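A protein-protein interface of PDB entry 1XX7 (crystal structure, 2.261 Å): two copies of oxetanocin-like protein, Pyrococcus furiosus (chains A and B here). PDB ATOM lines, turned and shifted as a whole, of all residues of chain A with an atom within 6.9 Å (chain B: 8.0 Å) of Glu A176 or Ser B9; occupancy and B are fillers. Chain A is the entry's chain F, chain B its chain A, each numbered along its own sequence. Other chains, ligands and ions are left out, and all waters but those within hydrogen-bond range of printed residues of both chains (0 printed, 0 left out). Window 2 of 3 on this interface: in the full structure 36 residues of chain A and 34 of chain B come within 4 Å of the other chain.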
ATOM      1  N   PHE A  47      34.306   6.915   7.400  1.00  0.00           N
ATOM      2  CA  PHE A  47      33.059   6.155   7.260  1.00  0.00           C
ATOM      3  C   PHE A  47      31.919   6.722   8.131  1.00  0.00           C
ATOM      4  O   PHE A  47      30.747   6.832   7.680  1.00  0.00           O
ATOM      5  CB  PHE A  47      33.270   4.668   7.607  1.00  0.00           C
ATOM      6  CG  PHE A  47      32.000   3.845   7.508  1.00  0.00           C
ATOM      7  CD1 PHE A  47      31.481   3.502   6.279  1.00  0.00           C
ATOM      8  CD2 PHE A  47      31.301   3.453   8.652  1.00  0.00           C
ATOM      9  CE1 PHE A  47      30.276   2.775   6.165  1.00  0.00           C
ATOM     10  CE2 PHE A  47      30.126   2.683   8.554  1.00  0.00           C
ATOM     11  CZ  PHE A  47      29.618   2.342   7.313  1.00  0.00           C
ATOM     12  N   LEU A  51      28.207   8.569   7.201  1.00  0.00           N
ATOM     13  CA  LEU A  51      26.958   8.250   7.877  1.00  0.00           C
ATOM     14  C   LEU A  51      26.308   9.467   8.545  1.00  0.00           C
ATOM     15  O   LEU A  51      25.128   9.715   8.407  1.00  0.00           O
ATOM     16  CB  LEU A  51      27.222   7.218   8.968  1.00  0.00           C
ATOM     17  CG  LEU A  51      26.828   5.779   8.722  1.00  0.00           C
ATOM     18  CD1 LEU A  51      27.248   5.288   7.348  1.00  0.00           C
ATOM     19  CD2 LEU A  51      27.421   4.993   9.800  1.00  0.00           C
ATOM     20  N   GLU A  55      22.873  11.425   7.475  1.00  0.00           N
ATOM     21  CA  GLU A  55      21.846  11.633   8.480  1.00  0.00           C
ATOM     22  C   GLU A  55      21.413  13.142   8.562  1.00  0.00           C
ATOM     23  O   GLU A  55      20.226  13.432   8.614  1.00  0.00           O
ATOM     24  CB  GLU A  55      22.335  11.114   9.827  1.00  0.00           C
ATOM     25  CG  GLU A  55      21.251  10.876  10.853  1.00  0.00           C
ATOM     26  CD  GLU A  55      20.107  10.003  10.300  1.00  0.00           C
ATOM     27  OE1 GLU A  55      20.377   8.840   9.863  1.00  0.00           O
ATOM     28  OE2 GLU A  55      18.946  10.497  10.283  1.00  0.00           O
ATOM     29  N   ILE A 138      33.689   3.914  20.532  1.00  0.00           N
ATOM     30  CA  ILE A 138      33.279   2.624  20.081  1.00  0.00           C
ATOM     31  C   ILE A 138      34.462   1.645  20.050  1.00  0.00           C
ATOM     32  O   ILE A 138      34.276   0.476  20.347  1.00  0.00           O
ATOM     33  CB  ILE A 138      32.586   2.722  18.725  1.00  0.00           C
ATOM     34  CG1 ILE A 138      31.250   3.478  18.878  1.00  0.00           C
ATOM     35  CG2 ILE A 138      32.325   1.349  18.162  1.00  0.00           C
ATOM     36  CD1 ILE A 138      30.688   4.042  17.574  1.00  0.00           C
ATOM     37  N   ARG A 171      20.746  12.422  17.655  1.00  0.00           N
ATOM     38  CA  ARG A 171      20.456  11.914  19.008  1.00  0.00           C
ATOM     39  C   ARG A 171      20.218  10.405  19.016  1.00  0.00           C
ATOM     40  O   ARG A 171      20.587   9.744  19.986  1.00  0.00           O
ATOM     41  CB  ARG A 171      19.287  12.682  19.667  1.00  0.00           C
ATOM     42  CG  ARG A 171      19.718  14.011  20.338  1.00  0.00           C
ATOM     43  N   GLU A 172      19.609   9.869  17.945  1.00  0.00           N
ATOM     44  CA  GLU A 172      19.490   8.416  17.738  1.00  0.00           C
ATOM     45  C   GLU A 172      20.842   7.695  17.872  1.00  0.00           C
ATOM     46  O   GLU A 172      20.951   6.717  18.614  1.00  0.00           O
ATOM     47  CB  GLU A 172      18.881   8.088  16.369  1.00  0.00           C
ATOM     48  N   ILE A 173      21.866   8.192  17.170  1.00  0.00           N
ATOM     49  CA  ILE A 173      23.190   7.560  17.178  1.00  0.00           C
ATOM     50  C   ILE A 173      23.913   7.773  18.498  1.00  0.00           C
ATOM     51  O   ILE A 173      24.523   6.848  19.016  1.00  0.00           O
ATOM     52  CB  ILE A 173      24.098   8.021  15.989  1.00  0.00           C
ATOM     53  CG1 ILE A 173      25.234   7.011  15.763  1.00  0.00           C
ATOM     54  CG2 ILE A 173      24.714   9.397  16.237  1.00  0.00           C
ATOM     55  N   ILE A 174      23.848   8.973  19.059  1.00  0.00           N
ATOM     56  CA  ILE A 174      24.537   9.224  20.318  1.00  0.00           C
ATOM     57  C   ILE A 174      23.929   8.386  21.474  1.00  0.00           C
ATOM     58  O   ILE A 174      24.643   8.014  22.413  1.00  0.00           O
ATOM     59  CB  ILE A 174      24.564  10.716  20.687  1.00  0.00           C
ATOM     60  CG1 ILE A 174      25.393  11.503  19.672  1.00  0.00           C
ATOM     61  CG2 ILE A 174      25.181  10.918  22.080  1.00  0.00           C
ATOM     62  CD1 ILE A 174      25.063  13.012  19.633  1.00  0.00           C
ATOM     63  N   GLU A 175      22.633   8.088  21.394  1.00  0.00           N
ATOM     64  CA  GLU A 175      21.978   7.264  22.404  1.00  0.00           C
ATOM     65  C   GLU A 175      22.322   5.788  22.195  1.00  0.00           C
ATOM     66  O   GLU A 175      22.467   5.061  23.168  1.00  0.00           O
ATOM     67  CB  GLU A 175      20.467   7.477  22.405  1.00  0.00           C
ATOM     68  N   GLU A 176      22.454   5.351  20.934  1.00  0.00           N
ATOM     69  CA  GLU A 176      22.923   3.982  20.619  1.00  0.00           C
ATOM     70  C   GLU A 176      24.323   3.718  21.171  1.00  0.00           C
ATOM     71  O   GLU A 176      24.615   2.621  21.620  1.00  0.00           O
ATOM     72  CB  GLU A 176      22.954   3.725  19.115  1.00  0.00           C
ATOM     73  CG  GLU A 176      21.626   3.412  18.485  1.00  0.00           C
ATOM     74  CD  GLU A 176      21.722   3.241  16.970  1.00  0.00           C
ATOM     75  OE1 GLU A 176      22.754   2.738  16.498  1.00  0.00           O
ATOM     76  OE2 GLU A 176      20.758   3.598  16.250  1.00  0.00           O
ATOM     77  N   VAL A 177      25.185   4.723  21.109  1.00  0.00           N
ATOM     78  CA  VAL A 177      26.533   4.608  21.639  1.00  0.00           C
ATOM     79  C   VAL A 177      26.517   4.610  23.163  1.00  0.00           C
ATOM     80  O   VAL A 177      27.300   3.894  23.794  1.00  0.00           O
ATOM     81  CB  VAL A 177      27.435   5.744  21.136  1.00  0.00           C
ATOM     82  CG1 VAL A 177      28.770   5.764  21.881  1.00  0.00           C
ATOM     83  CG2 VAL A 177      27.655   5.602  19.639  1.00  0.00           C
ATOM     84  N   ARG A 178      25.649   5.425  23.758  1.00  0.00           N
ATOM     85  CA  ARG A 178      25.510   5.436  25.208  1.00  0.00           C
ATOM     86  C   ARG A 178      25.073   4.056  25.693  1.00  0.00           C
ATOM     87  O   ARG A 178      25.670   3.497  26.611  1.00  0.00           O
ATOM     88  CB  ARG A 178      24.521   6.513  25.661  1.00  0.00           C
ATOM     89  CG  ARG A 178      24.527   6.736  27.174  1.00  0.00           C
ATOM     90  CD  ARG A 178      23.720   7.943  27.569  1.00  0.00           C
ATOM     91  NE  ARG A 178      24.503   9.192  27.586  1.00  0.00           N
ATOM     92  CZ  ARG A 178      24.385  10.212  26.711  1.00  0.00           C
ATOM     93  NH1 ARG A 178      23.532  10.154  25.680  1.00  0.00           N
ATOM     94  NH2 ARG A 178      25.132  11.311  26.862  1.00  0.00           N
ATOM     95  N   ARG A 179      24.058   3.500  25.036  1.00  0.00           N
ATOM     96  CA  ARG A 179      23.576   2.167  25.340  1.00  0.00           C
ATOM     97  C   ARG A 179      24.683   1.072  25.350  1.00  0.00           C
ATOM     98  O   ARG A 179      24.575   0.113  26.120  1.00  0.00           O
ATOM     99  CB  ARG A 179      22.411   1.798  24.415  1.00  0.00           C
ATOM    100  CG  ARG A 179      21.126   2.567  24.746  1.00  0.00           C
ATOM    101  N   LEU A 180      25.736   1.209  24.525  1.00  0.00           N
ATOM    102  CA  LEU A 180      26.979   0.442  24.761  1.00  0.00           C
ATOM    103  C   LEU A 180      27.601   1.012  26.045  1.00  0.00           C
ATOM    104  O   LEU A 180      27.841   0.295  27.003  1.00  0.00           O
ATOM    105  CB  LEU A 180      28.015   0.540  23.609  1.00  0.00           C
ATOM    106  CG  LEU A 180      27.677   0.375  22.110  1.00  0.00           C
ATOM    107  CD1 LEU A 180      28.886   0.829  21.264  1.00  0.00           C
ATOM    108  CD2 LEU A 180      27.239  -1.037  21.710  1.00  0.00           C
ATOM    109  N   SER B   9      23.596   4.193  13.086  1.00  0.00           N
ATOM    110  CA  SER B   9      23.550   2.750  13.519  1.00  0.00           C
ATOM    111  C   SER B   9      24.964   2.288  13.897  1.00  0.00           C
ATOM    112  O   SER B   9      25.902   2.332  13.055  1.00  0.00           O
ATOM    113  CB  SER B   9      22.952   1.862  12.414  1.00  0.00           C
ATOM    114  OG  SER B   9      22.464   0.617  12.903  1.00  0.00           O
ATOM    115  N   ILE B  10      25.100   1.886  15.169  1.00  0.00           N
ATOM    116  CA  ILE B  10      26.330   1.335  15.732  1.00  0.00           C
ATOM    117  C   ILE B  10      26.779   0.046  15.013  1.00  0.00           C
ATOM    118  O   ILE B  10      27.977  -0.219  14.937  1.00  0.00           O
ATOM    119  CB  ILE B  10      26.216   1.160  17.313  1.00  0.00           C
ATOM    120  CG1 ILE B  10      26.449   2.485  18.020  1.00  0.00           C
ATOM    121  CG2 ILE B  10      27.255   0.235  17.893  1.00  0.00           C
ATOM    122  N   ASP B  11      25.823  -0.702  14.452  1.00  0.00           N
ATOM    123  CA  ASP B  11      26.097  -1.950  13.723  1.00  0.00           C
ATOM    124  C   ASP B  11      26.893  -1.718  12.471  1.00  0.00           C
ATOM    125  O   ASP B  11      27.819  -2.470  12.186  1.00  0.00           O
ATOM    126  CB  ASP B  11      24.803  -2.723  13.365  1.00  0.00           C
ATOM    127  CG  ASP B  11      24.230  -3.524  14.560  1.00  0.00           C
ATOM    128  OD1 ASP B  11      24.885  -3.621  15.631  1.00  0.00           O
ATOM    129  OD2 ASP B  11      23.108  -4.077  14.430  1.00  0.00           O
ATOM    130  N   LEU B  12      26.528  -0.695  11.703  1.00  0.00           N
ATOM    131  CA  LEU B  12      27.312  -0.305  10.558  1.00  0.00           C
ATOM    132  C   LEU B  12      28.756   0.027  10.965  1.00  0.00           C
ATOM    133  O   LEU B  12      29.696  -0.331  10.295  1.00  0.00           O
ATOM    134  CB  LEU B  12      26.672   0.873   9.856  1.00  0.00           C
ATOM    135  CG  LEU B  12      25.441   0.477   9.023  1.00  0.00           C
ATOM    136  CD1 LEU B  12      24.760   1.735   8.501  1.00  0.00           C
ATOM    137  CD2 LEU B  12      25.838  -0.445   7.844  1.00  0.00           C
ATOM    138  N   ILE B  13      28.907   0.690  12.091  1.00  0.00           N
ATOM    139  CA  ILE B  13      30.186   1.219  12.496  1.00  0.00           C
ATOM    140  C   ILE B  13      31.059   0.074  13.016  1.00  0.00           C
ATOM    141  O   ILE B  13      32.234   0.025  12.722  1.00  0.00           O
ATOM    142  CB  ILE B  13      29.988   2.360  13.540  1.00  0.00           C
ATOM    143  CG1 ILE B  13      29.439   3.582  12.820  1.00  0.00           C
ATOM    144  CG2 ILE B  13      31.255   2.706  14.201  1.00  0.00           C
ATOM    145  CD1 ILE B  13      28.889   4.642  13.699  1.00  0.00           C
ATOM    146  N   LEU B  14      30.448  -0.825  13.776  1.00  0.00           N
ATOM    147  CA  LEU B  14      31.043  -2.098  14.193  1.00  0.00           C
ATOM    148  C   LEU B  14      31.466  -2.935  12.988  1.00  0.00           C
ATOM    149  O   LEU B  14      32.552  -3.523  12.974  1.00  0.00           O
ATOM    150  CB  LEU B  14      30.051  -2.875  15.077  1.00  0.00           C
ATOM    151  CG  LEU B  14      29.869  -2.280  16.481  1.00  0.00           C
ATOM    152  CD1 LEU B  14      28.701  -2.960  17.225  1.00  0.00           C
ATOM    153  CD2 LEU B  14      31.122  -2.394  17.310  1.00  0.00           C
ATOM    154  N   LEU B  15      30.618  -2.963  11.970  1.00  0.00           N
ATOM    155  CA  LEU B  15      30.975  -3.597  10.708  1.00  0.00           C
ATOM    156  C   LEU B  15      32.246  -3.028  10.073  1.00  0.00           C
ATOM    157  O   LEU B  15      33.127  -3.778   9.738  1.00  0.00           O
ATOM    158  CB  LEU B  15      29.831  -3.503   9.718  1.00  0.00           C
ATOM    159  CG  LEU B  15      30.046  -4.450   8.528  1.00  0.00           C
ATOM    160  CD1 LEU B  15      29.722  -5.894   8.964  1.00  0.00           C
ATOM    161  CD2 LEU B  15      29.222  -4.074   7.402  1.00  0.00           C
ATOM    162  N   VAL B 106      23.438  -4.996   3.893  1.00  0.00           N
ATOM    163  CA  VAL B 106      23.721  -4.075   5.002  1.00  0.00           C
ATOM    164  C   VAL B 106      23.623  -2.593   4.674  1.00  0.00           C
ATOM    165  O   VAL B 106      23.180  -1.806   5.515  1.00  0.00           O
ATOM    166  CB  VAL B 106      25.122  -4.316   5.628  1.00  0.00           C
ATOM    167  CG1 VAL B 106      25.161  -5.659   6.336  1.00  0.00           C
ATOM    168  CG2 VAL B 106      26.261  -4.154   4.597  1.00  0.00           C
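No position is printed for both chains.
Phe A47 touches Leu B12. Leu A51 touches Ile B13 (CD2 to CG1, 3.9 Å). CD1 of Ile A138 touches CG2 of Ile B13, at 3.7 Å. Ser B9 touches Glu A176. Val A177 touches Ile B10. Leu A180 touches Ile B10.
Glu A176 touches just these residues of chain B: Ser B9 (3.1 Å) and Ile B10 (2.8 Å). Ser B9 touches just one residue of chain A: Glu A176. No residue of chain B comes within 4 Å of Glu A175. Printed residues of chain B within 4 Å of Ile A138: Ile B13. Printed residues of chain A within 4 Å of Ile B13: Leu A51 (3.9 Å) and Ile A138 (3.7 Å). Of the printed residues of chain A, Leu B12 touches Phe A47 (3.5 Å). Of the printed residues of chain B, Leu A180 touches Ile B10 (3.8 Å). Printed residues of chain A within 4 Å of Ile B10: Glu A176, Val A177 and Leu A180.
Of the 14 printed residues of chain A, 6 touch a printed residue of chain B. Hydrophobic or aromatic side chains of chain A within 4 Å of the printed part of chain B: Phe A47, Leu A51, Ile A138, Val A177 and Leu A180. Along chain B the printed residues that touch a printed residue of chain A span positions 9 to 13. Among the printed residues, 7 pairs touch across the chains. Among the printed residues, no Asp or Glu carboxylate lies within 4 Å of a Lys or Arg side-chain nitrogen of the other chain.
The backbone NH (N) of Ile B10 sits at hydrogen-bond distance from the side-chain carboxylate (OE1) of Glu A176 (2.8 Å).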
